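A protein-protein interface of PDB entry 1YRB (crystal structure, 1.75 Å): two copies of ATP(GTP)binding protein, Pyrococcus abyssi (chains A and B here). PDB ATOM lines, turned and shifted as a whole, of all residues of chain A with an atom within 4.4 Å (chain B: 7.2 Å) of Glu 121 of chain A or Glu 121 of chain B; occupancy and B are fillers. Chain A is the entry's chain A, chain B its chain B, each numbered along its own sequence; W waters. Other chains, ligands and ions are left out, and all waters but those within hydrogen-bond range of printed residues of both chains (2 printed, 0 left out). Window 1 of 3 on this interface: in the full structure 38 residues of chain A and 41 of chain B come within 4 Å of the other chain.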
ATOM      1  N   THR A  22      24.164 -22.304  15.679  1.00  0.00           N
ATOM      2  CA  THR A  22      22.865 -22.930  15.963  1.00  0.00           C
ATOM      3  C   THR A  22      22.148 -23.324  14.681  1.00  0.00           C
ATOM      4  O   THR A  22      22.457 -22.820  13.605  1.00  0.00           O
ATOM      5  CB  THR A  22      21.936 -22.014  16.802  1.00  0.00           C
ATOM      6  OG1 THR A  22      20.802 -22.781  17.231  1.00  0.00           O
ATOM      7  CG2 THR A  22      21.440 -20.884  15.969  1.00  0.00           C
ATOM      8  N   ALA A  23      21.187 -24.238  14.778  1.00  0.00           N
ATOM      9  CA  ALA A  23      20.463 -24.640  13.578  1.00  0.00           C
ATOM     10  C   ALA A  23      19.898 -23.438  12.837  1.00  0.00           C
ATOM     11  O   ALA A  23      19.272 -22.573  13.433  1.00  0.00           O
ATOM     12  CB  ALA A  23      19.339 -25.624  13.926  1.00  0.00           C
ATOM     13  N   GLY A 118      23.530 -30.158  12.454  1.00  0.00           N
ATOM     14  CA  GLY A 118      22.673 -28.982  12.321  1.00  0.00           C
ATOM     15  C   GLY A 118      22.461 -28.324  13.677  1.00  0.00           C
ATOM     16  O   GLY A 118      22.442 -27.102  13.796  1.00  0.00           O
ATOM     17  N   GLN A 119      22.283 -29.155  14.694  1.00  0.00           N
ATOM     18  CA  GLN A 119      22.152 -28.656  16.054  1.00  0.00           C
ATOM     19  C   GLN A 119      23.531 -28.561  16.677  1.00  0.00           C
ATOM     20  O   GLN A 119      24.193 -29.563  16.895  1.00  0.00           O
ATOM     21  CB  GLN A 119      21.264 -29.567  16.899  1.00  0.00           C
ATOM     22  CG  GLN A 119      19.860 -29.770  16.339  1.00  0.00           C
ATOM     23  CD  GLN A 119      18.988 -28.536  16.435  1.00  0.00           C
ATOM     24  OE1 GLN A 119      19.264 -27.615  17.215  1.00  0.00           O
ATOM     25  NE2 GLN A 119      17.912 -28.515  15.650  1.00  0.00           N
ATOM     26  N   MET A 120      23.951 -27.342  16.983  1.00  0.00           N
ATOM     27  CA  MET A 120      25.242 -27.122  17.626  1.00  0.00           C
ATOM     28  C   MET A 120      25.435 -27.950  18.921  1.00  0.00           C
ATOM     29  O   MET A 120      26.543 -28.372  19.255  1.00  0.00           O
ATOM     30  CB  MET A 120      25.349 -25.634  17.912  1.00  0.00           C
ATOM     31  CG  MET A 120      26.513 -25.201  18.713  1.00  0.00           C
ATOM     32  SD  MET A 120      26.563 -23.411  18.563  1.00  0.00           S
ATOM     33  CE  MET A 120      24.926 -22.932  19.107  1.00  0.00           C
ATOM     34  N   GLU A 121      24.361 -28.185  19.662  1.00  0.00           N
ATOM     35  CA  GLU A 121      24.522 -28.929  20.913  1.00  0.00           C
ATOM     36  C   GLU A 121      24.872 -30.385  20.648  1.00  0.00           C
ATOM     37  O   GLU A 121      25.454 -31.051  21.496  1.00  0.00           O
ATOM     38  CB  GLU A 121      23.270 -28.807  21.784  1.00  0.00           C
ATOM     39  CG  GLU A 121      22.035 -29.368  21.144  1.00  0.00           C
ATOM     40  CD  GLU A 121      20.798 -28.772  21.775  1.00  0.00           C
ATOM     41  OE1 GLU A 121      20.259 -29.399  22.701  1.00  0.00           O
ATOM     42  OE2 GLU A 121      20.407 -27.659  21.369  1.00  0.00           O
ATOM     43  N   THR A 122      24.534 -30.890  19.460  1.00  0.00           N
ATOM     44  CA  THR A 122      24.917 -32.251  19.137  1.00  0.00           C
ATOM     45  C   THR A 122      26.437 -32.278  19.063  1.00  0.00           C
ATOM     46  O   THR A 122      27.072 -33.238  19.500  1.00  0.00           O
ATOM     47  CB  THR A 122      24.299 -32.749  17.800  1.00  0.00           C
ATOM     48  OG1 THR A 122      22.884 -32.492  17.786  1.00  0.00           O
ATOM     49  CG2 THR A 122      24.523 -34.244  17.669  1.00  0.00           C
ATOM     50  N   PHE A 123      27.026 -31.202  18.545  1.00  0.00           N
ATOM     51  CA  PHE A 123      28.462 -31.166  18.333  1.00  0.00           C
ATOM     52  C   PHE A 123      29.190 -30.894  19.645  1.00  0.00           C
ATOM     53  O   PHE A 123      30.225 -31.505  19.936  1.00  0.00           O
ATOM     54  CB  PHE A 123      28.831 -30.110  17.270  1.00  0.00           C
ATOM     55  CG  PHE A 123      30.217 -30.301  16.671  1.00  0.00           C
ATOM     56  CD1 PHE A 123      30.519 -31.441  15.933  1.00  0.00           C
ATOM     57  CD2 PHE A 123      31.197 -29.327  16.829  1.00  0.00           C
ATOM     58  CE1 PHE A 123      31.784 -31.616  15.382  1.00  0.00           C
ATOM     59  CE2 PHE A 123      32.456 -29.497  16.285  1.00  0.00           C
ATOM     60  CZ  PHE A 123      32.748 -30.642  15.560  1.00  0.00           C
ATOM     61  N   LEU A 124      28.639 -29.993  20.453  1.00  0.00           N
ATOM     62  CA  LEU A 124      29.323 -29.545  21.662  1.00  0.00           C
ATOM     63  C   LEU A 124      29.051 -30.438  22.867  1.00  0.00           C
ATOM     64  O   LEU A 124      29.857 -30.460  23.800  1.00  0.00           O
ATOM     65  CB  LEU A 124      28.917 -28.112  22.008  1.00  0.00           C
ATOM     66  CG  LEU A 124      29.237 -27.038  20.982  1.00  0.00           C
ATOM     67  CD1 LEU A 124      28.714 -25.696  21.506  1.00  0.00           C
ATOM     68  CD2 LEU A 124      30.738 -26.978  20.734  1.00  0.00           C
ATOM     69  N   PHE A 125      27.918 -31.146  22.855  1.00  0.00           N
ATOM     70  CA  PHE A 125      27.510 -31.971  24.009  1.00  0.00           C
ATOM     71  C   PHE A 125      27.518 -33.475  23.763  1.00  0.00           C
ATOM     72  O   PHE A 125      27.225 -34.260  24.672  1.00  0.00           O
ATOM     73  CB  PHE A 125      26.135 -31.525  24.514  1.00  0.00           C
ATOM     74  CG  PHE A 125      26.157 -30.187  25.167  1.00  0.00           C
ATOM     75  CD1 PHE A 125      26.295 -30.080  26.547  1.00  0.00           C
ATOM     76  CD2 PHE A 125      26.086 -29.024  24.414  1.00  0.00           C
ATOM     77  CE1 PHE A 125      26.331 -28.843  27.153  1.00  0.00           C
ATOM     78  CE2 PHE A 125      26.129 -27.791  25.013  1.00  0.00           C
ATOM     79  CZ  PHE A 125      26.255 -27.699  26.395  1.00  0.00           C
ATOM     80  N   HIS A 126      27.841 -33.887  22.546  1.00  0.00           N
ATOM     81  CA  HIS A 126      27.960 -35.290  22.222  1.00  0.00           C
ATOM     82  C   HIS A 126      29.425 -35.666  22.048  1.00  0.00           C
ATOM     83  O   HIS A 126      30.226 -34.869  21.572  1.00  0.00           O
ATOM     84  CB  HIS A 126      27.200 -35.618  20.937  1.00  0.00           C
ATOM     85  CG  HIS A 126      26.972 -37.083  20.733  1.00  0.00           C
ATOM     86  ND1 HIS A 126      27.932 -37.928  20.205  1.00  0.00           N
ATOM     87  CD2 HIS A 126      25.892 -37.856  20.988  1.00  0.00           C
ATOM     88  CE1 HIS A 126      27.452 -39.156  20.151  1.00  0.00           C
ATOM     89  NE2 HIS A 126      26.216 -39.139  20.623  1.00  0.00           N
ATOM     90  N   VAL B  20      15.604 -27.144  31.431  1.00  0.00           N
ATOM     91  CA  VAL B  20      16.350 -26.862  30.209  1.00  0.00           C
ATOM     92  C   VAL B  20      17.544 -27.791  30.209  1.00  0.00           C
ATOM     93  O   VAL B  20      18.075 -28.123  31.265  1.00  0.00           O
ATOM     94  CB  VAL B  20      16.855 -25.389  30.164  1.00  0.00           C
ATOM     95  CG1 VAL B  20      17.846 -25.187  29.024  1.00  0.00           C
ATOM     96  CG2 VAL B  20      15.689 -24.425  30.006  1.00  0.00           C
ATOM     97  N   GLY B  21      17.959 -28.217  29.028  1.00  0.00           N
ATOM     98  CA  GLY B  21      19.060 -29.168  28.953  1.00  0.00           C
ATOM     99  C   GLY B  21      19.173 -29.655  27.521  1.00  0.00           C
ATOM    100  O   GLY B  21      18.273 -29.452  26.688  1.00  0.00           O
ATOM    101  N   THR B  22      20.298 -30.272  27.197  1.00  0.00           N
ATOM    102  CA  THR B  22      20.471 -30.709  25.827  1.00  0.00           C
ATOM    103  C   THR B  22      19.503 -31.844  25.509  1.00  0.00           C
ATOM    104  O   THR B  22      18.944 -32.474  26.403  1.00  0.00           O
ATOM    105  CB  THR B  22      21.914 -31.132  25.524  1.00  0.00           C
ATOM    106  OG1 THR B  22      22.074 -31.219  24.090  1.00  0.00           O
ATOM    107  CG2 THR B  22      22.205 -32.465  26.191  1.00  0.00           C
ATOM    108  N   ALA B  23      19.297 -32.100  24.230  1.00  0.00           N
ATOM    109  CA  ALA B  23      18.335 -33.115  23.848  1.00  0.00           C
ATOM    110  C   ALA B  23      18.737 -34.431  24.480  1.00  0.00           C
ATOM    111  O   ALA B  23      19.901 -34.823  24.406  1.00  0.00           O
ATOM    112  CB  ALA B  23      18.249 -33.238  22.313  1.00  0.00           C
ATOM    113  N   GLY B  24      17.774 -35.130  25.091  1.00  0.00           N
ATOM    114  CA  GLY B  24      18.054 -36.419  25.722  1.00  0.00           C
ATOM    115  C   GLY B  24      18.507 -36.377  27.167  1.00  0.00           C
ATOM    116  O   GLY B  24      18.714 -37.422  27.772  1.00  0.00           O
ATOM    117  N   LYS B  27      14.619 -33.730  30.261  1.00  0.00           N
ATOM    118  CA  LYS B  27      13.707 -32.624  30.593  1.00  0.00           C
ATOM    119  C   LYS B  27      12.277 -33.134  30.738  1.00  0.00           C
ATOM    120  O   LYS B  27      11.573 -32.808  31.695  1.00  0.00           O
ATOM    121  CB  LYS B  27      13.696 -31.572  29.492  1.00  0.00           C
ATOM    122  CG  LYS B  27      15.049 -30.865  29.315  1.00  0.00           C
ATOM    123  CD  LYS B  27      15.004 -29.876  28.162  1.00  0.00           C
ATOM    124  CE  LYS B  27      14.830 -30.547  26.793  1.00  0.00           C
ATOM    125  NZ  LYS B  27      16.071 -31.257  26.350  1.00  0.00           N
ATOM    126  N   PRO B 117      11.696 -26.890  24.456  1.00  0.00           N
ATOM    127  CA  PRO B 117      12.048 -27.560  23.201  1.00  0.00           C
ATOM    128  C   PRO B 117      13.167 -28.592  23.420  1.00  0.00           C
ATOM    129  O   PRO B 117      14.039 -28.409  24.272  1.00  0.00           O
ATOM    130  CB  PRO B 117      12.521 -26.411  22.309  1.00  0.00           C
ATOM    131  CG  PRO B 117      11.758 -25.202  22.817  1.00  0.00           C
ATOM    132  CD  PRO B 117      11.612 -25.426  24.309  1.00  0.00           C
ATOM    133  N   GLY B 118      13.144 -29.699  22.675  1.00  0.00           N
ATOM    134  CA  GLY B 118      14.073 -30.777  22.978  1.00  0.00           C
ATOM    135  C   GLY B 118      15.527 -30.358  22.812  1.00  0.00           C
ATOM    136  O   GLY B 118      16.394 -30.799  23.542  1.00  0.00           O
ATOM    137  N   GLN B 119      15.773 -29.471  21.860  1.00  0.00           N
ATOM    138  CA  GLN B 119      17.102 -28.893  21.691  1.00  0.00           C
ATOM    139  C   GLN B 119      17.137 -27.588  22.440  1.00  0.00           C
ATOM    140  O   GLN B 119      16.381 -26.680  22.114  1.00  0.00           O
ATOM    141  CB  GLN B 119      17.366 -28.602  20.215  1.00  0.00           C
ATOM    142  CG  GLN B 119      17.065 -29.781  19.295  1.00  0.00           C
ATOM    143  CD  GLN B 119      18.165 -30.792  19.323  1.00  0.00           C
ATOM    144  OE1 GLN B 119      19.262 -30.510  19.805  1.00  0.00           O
ATOM    145  NE2 GLN B 119      17.887 -31.981  18.812  1.00  0.00           N
ATOM    146  N   MET B 120      18.004 -27.477  23.430  1.00  0.00           N
ATOM    147  CA  MET B 120      17.970 -26.269  24.230  1.00  0.00           C
ATOM    148  C   MET B 120      18.345 -25.058  23.391  1.00  0.00           C
ATOM    149  O   MET B 120      17.896 -23.947  23.658  1.00  0.00           O
ATOM    150  CB  MET B 120      18.809 -26.398  25.489  1.00  0.00           C
ATOM    151  CG  MET B 120      20.298 -26.451  25.285  1.00  0.00           C
ATOM    152  SD  MET B 120      21.104 -26.536  26.896  1.00  0.00           S
ATOM    153  CE  MET B 120      22.610 -27.343  26.380  1.00  0.00           C
ATOM    154  N   GLU B 121      19.119 -25.270  22.331  1.00  0.00           N
ATOM    155  CA  GLU B 121      19.435 -24.142  21.463  1.00  0.00           C
ATOM    156  C   GLU B 121      18.210 -23.553  20.777  1.00  0.00           C
ATOM    157  O   GLU B 121      18.189 -22.367  20.470  1.00  0.00           O
ATOM    158  CB  GLU B 121      20.530 -24.496  20.447  1.00  0.00           C
ATOM    159  CG  GLU B 121      20.103 -25.366  19.300  1.00  0.00           C
ATOM    160  CD  GLU B 121      21.309 -26.021  18.670  1.00  0.00           C
ATOM    161  OE1 GLU B 121      21.703 -25.583  17.565  1.00  0.00           O
ATOM    162  OE2 GLU B 121      21.880 -26.922  19.325  1.00  0.00           O
ATOM    163  N   THR B 122      17.173 -24.355  20.564  1.00  0.00           N
ATOM    164  CA  THR B 122      15.968 -23.812  19.974  1.00  0.00           C
ATOM    165  C   THR B 122      15.328 -22.848  20.954  1.00  0.00           C
ATOM    166  O   THR B 122      14.678 -21.900  20.542  1.00  0.00           O
ATOM    167  CB  THR B 122      14.947 -24.888  19.607  1.00  0.00           C
ATOM    168  OG1 THR B 122      15.626 -25.982  18.981  1.00  0.00           O
ATOM    169  CG2 THR B 122      13.930 -24.328  18.635  1.00  0.00           C
ATOM    170  N   PHE B 123      15.517 -23.105  22.242  1.00  0.00           N
ATOM    171  CA  PHE B 123      14.935 -22.297  23.301  1.00  0.00           C
ATOM    172  C   PHE B 123      15.788 -21.067  23.569  1.00  0.00           C
ATOM    173  O   PHE B 123      15.259 -19.992  23.824  1.00  0.00           O
ATOM    174  CB  PHE B 123      14.803 -23.125  24.586  1.00  0.00           C
ATOM    175  CG  PHE B 123      13.915 -22.491  25.640  1.00  0.00           C
ATOM    176  CD1 PHE B 123      12.578 -22.245  25.378  1.00  0.00           C
ATOM    177  CD2 PHE B 123      14.417 -22.189  26.895  1.00  0.00           C
ATOM    178  CE1 PHE B 123      11.754 -21.660  26.352  1.00  0.00           C
ATOM    179  CE2 PHE B 123      13.608 -21.613  27.860  1.00  0.00           C
ATOM    180  CZ  PHE B 123      12.269 -21.374  27.583  1.00  0.00           C
ATOM    181  N   LEU B 124      17.106 -21.222  23.498  1.00  0.00           N
ATOM    182  CA  LEU B 124      18.025 -20.119  23.812  1.00  0.00           C
ATOM    183  C   LEU B 124      18.225 -19.137  22.663  1.00  0.00           C
ATOM    184  O   LEU B 124      18.507 -17.964  22.909  1.00  0.00           O
ATOM    185  CB  LEU B 124      19.389 -20.675  24.244  1.00  0.00           C
ATOM    186  CG  LEU B 124      19.342 -21.571  25.479  1.00  0.00           C
ATOM    187  CD1 LEU B 124      20.688 -22.312  25.700  1.00  0.00           C
ATOM    188  CD2 LEU B 124      18.954 -20.770  26.719  1.00  0.00           C
ATOM    189  N   PHE B 125      18.089 -19.612  21.421  1.00  0.00           N
ATOM    190  CA  PHE B 125      18.434 -18.805  20.243  1.00  0.00           C
ATOM    191  C   PHE B 125      17.244 -18.402  19.393  1.00  0.00           C
ATOM    192  O   PHE B 125      17.413 -17.692  18.397  1.00  0.00           O
ATOM    193  CB  PHE B 125      19.472 -19.530  19.364  1.00  0.00           C
ATOM    194  CG  PHE B 125      20.826 -19.651  19.995  1.00  0.00           C
ATOM    195  CD1 PHE B 125      21.825 -18.726  19.699  1.00  0.00           C
ATOM    196  CD2 PHE B 125      21.111 -20.682  20.879  1.00  0.00           C
ATOM    197  CE1 PHE B 125      23.081 -18.834  20.272  1.00  0.00           C
ATOM    198  CE2 PHE B 125      22.355 -20.797  21.473  1.00  0.00           C
ATOM    199  CZ  PHE B 125      23.344 -19.866  21.175  1.00  0.00           C
ATOM    200  N   HIS B 126      16.041 -18.828  19.760  1.00  0.00           N
ATOM    201  CA  HIS B 126      14.854 -18.417  19.024  1.00  0.00           C
ATOM    202  C   HIS B 126      14.100 -17.368  19.830  1.00  0.00           C
ATOM    203  O   HIS B 126      14.097 -17.412  21.065  1.00  0.00           O
ATOM    204  CB  HIS B 126      13.943 -19.613  18.738  1.00  0.00           C
ATOM    205  CG  HIS B 126      12.883 -19.340  17.713  1.00  0.00           C
ATOM    206  ND1 HIS B 126      11.673 -18.740  18.019  1.00  0.00           N
ATOM    207  CD2 HIS B 126      12.851 -19.597  16.384  1.00  0.00           C
ATOM    208  CE1 HIS B 126      10.948 -18.639  16.924  1.00  0.00           C
ATOM    209  NE2 HIS B 126      11.639 -19.148  15.915  1.00  0.00           N
ATOM    210  N   PHE B 162      28.399 -22.800  31.213  1.00  0.00           N
ATOM    211  CA  PHE B 162      27.213 -22.791  30.363  1.00  0.00           C
ATOM    212  C   PHE B 162      25.986 -22.346  31.154  1.00  0.00           C
ATOM    213  O   PHE B 162      25.169 -21.573  30.668  1.00  0.00           O
ATOM    214  CB  PHE B 162      26.990 -24.168  29.735  1.00  0.00           C
ATOM    215  CG  PHE B 162      26.116 -24.138  28.523  1.00  0.00           C
ATOM    216  CD1 PHE B 162      26.659 -23.961  27.268  1.00  0.00           C
ATOM    217  CD2 PHE B 162      24.764 -24.294  28.637  1.00  0.00           C
ATOM    218  CE1 PHE B 162      25.846 -23.944  26.137  1.00  0.00           C
ATOM    219  CE2 PHE B 162      23.943 -24.259  27.514  1.00  0.00           C
ATOM    220  CZ  PHE B 162      24.487 -24.083  26.275  1.00  0.00           C
HETATM  221  O   HOH W   1      20.793 -32.736  19.833  1.00  0.00           O
HETATM  222  O   HOH W   2      17.275 -25.511  16.884  1.00  0.00           O
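Among the printed residues, merely in contact across the chains: Gln 119 of chain A with Gln 119 of chain B, Phe 125 of chain A with Met 120 of chain B and Phe 125 of chain A with Phe 162 of chain B.
Along chain B the printed residues that touch a printed residue of chain A span positions 22 to 162.
Printed residues of chain A that touch a printed residue of chain B: Thr 22, Ala 23, Gln 119, Met 120, Glu 121 and Phe 125.
Water W1 lies within hydrogen-bond range of OE1 of Gln 119 of chain B and OG1 of Thr 122 of chain A.
Water W2 lies within hydrogen-bond range of OG1 of Thr 122 of chain B and OE1 of Gln 119 of chain A.
Thr 22 of chain A touches Glu 121 of chain B, and with the chains exchanged Glu 121 of chain A touches Thr 22 of chain B.
Ala 23 of chain A touches Glu 121 of chain B, and with the chains exchanged Glu 121 of chain A touches Ala 23 of chain B.
Gln 119 of chain A touches its own counterpart, Gln 119 of chain B.
Met 120 of chain A touches Glu 121 of chain B, and with the chains exchanged Glu 121 of chain A touches Met 120 of chain B.
11 positions are printed for both chains.
Of the 12 pairs that touch across the chains among the printed residues, 10 have their exchanged pair printed and touching as well.
Glu 121 of chain A touches just these residues of chain B: Thr 22, Ala 23, Gln 119, Met 120 and Glu 121.
Printed residues of chain A within 4 Å of Met 120 of chain B: Glu 121 and Phe 125.
Of the printed residues of chain B, Gln 119 of chain A touches Gln 119 and Glu 121.
Of the printed residues of chain B, Thr 22 of chain A touches Glu 121 (3.0 Å).
Of the printed residues of chain B, Met 120 of chain A touches Glu 121.
Gly 118 of chain A touches none of the printed residues of chain B.
The nearest residue of chain B that does not touch Glu 121 of chain A is Gly 118 of chain B (4.2 Å).
The nearest residue of chain A that does not touch Glu 121 of chain B is Gly 118 of chain A (4.1 Å).
The nearest printed residue of chain A that does not touch Thr 22 of chain B is Phe 125 of chain A (4.1 Å).
OG1 of Thr 22 of chain A lies within hydrogen-bond range of OE1 of Glu 121 of chain B, at 3.0 Å.
The side-chain carboxylate (OE1) of Glu 121 of chain B lies within hydrogen-bond range of the backbone NH (N) of Ala 23 of chain A, at 3.1 Å.
The side-chain amide oxygen of Gln 119 of chain A lies close to the side-chain carboxylate of Glu 121 of chain B (3.2 Å).
N of Met 120 of chain A is in hydrogen-bond range of OE1 of Glu 121 of chain B (2.9 Å).
The side-chain carboxylate of Glu 121 of chain A is in hydrogen-bond range of the side-chain hydroxyl of Thr 22 of chain B (2.9 Å).
The side-chain carboxylate of Glu 121 of chain A is in hydrogen-bond range of the backbone NH of Ala 23 of chain B (3.2 Å).
OE1 of Glu 121 of chain A lies close to OE1 of Gln 119 of chain B (3.3 Å).
N of Met 120 of chain B sits at hydrogen-bond distance from OE1 of Glu 121 of chain A (3.1 Å).
The side-chain carboxylate (OE2) of Glu 121 of chain B is in hydrogen-bond range of the backbone NH (N) of Glu 121 of chain A (2.8 Å).
The backbone NH of Ala 23 of chain A sits close to the backbone carbonyl oxygen of Gly 118 of chain A, at 3.3 Å.
The side-chain hydroxyl (OG1) of Thr 122 of chain A lies close to the backbone carbonyl oxygen (O) of Gln 119 of chain A, 3.3 Å away.
The backbone carbonyl oxygen (O) of Thr 22 of chain B sits at hydrogen-bond distance from the side-chain amino group (NZ) of Lys 27 of chain B (3.1 Å).
The backbone carbonyl oxygen (O) of Gly 118 of chain B lies close to the backbone NH (N) of Ala 23 of chain B.
The side-chain hydroxyl of Thr 122 of chain B lies within hydrogen-bond range of the backbone carbonyl oxygen of Gln 119 of chain B (3.3 Å).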
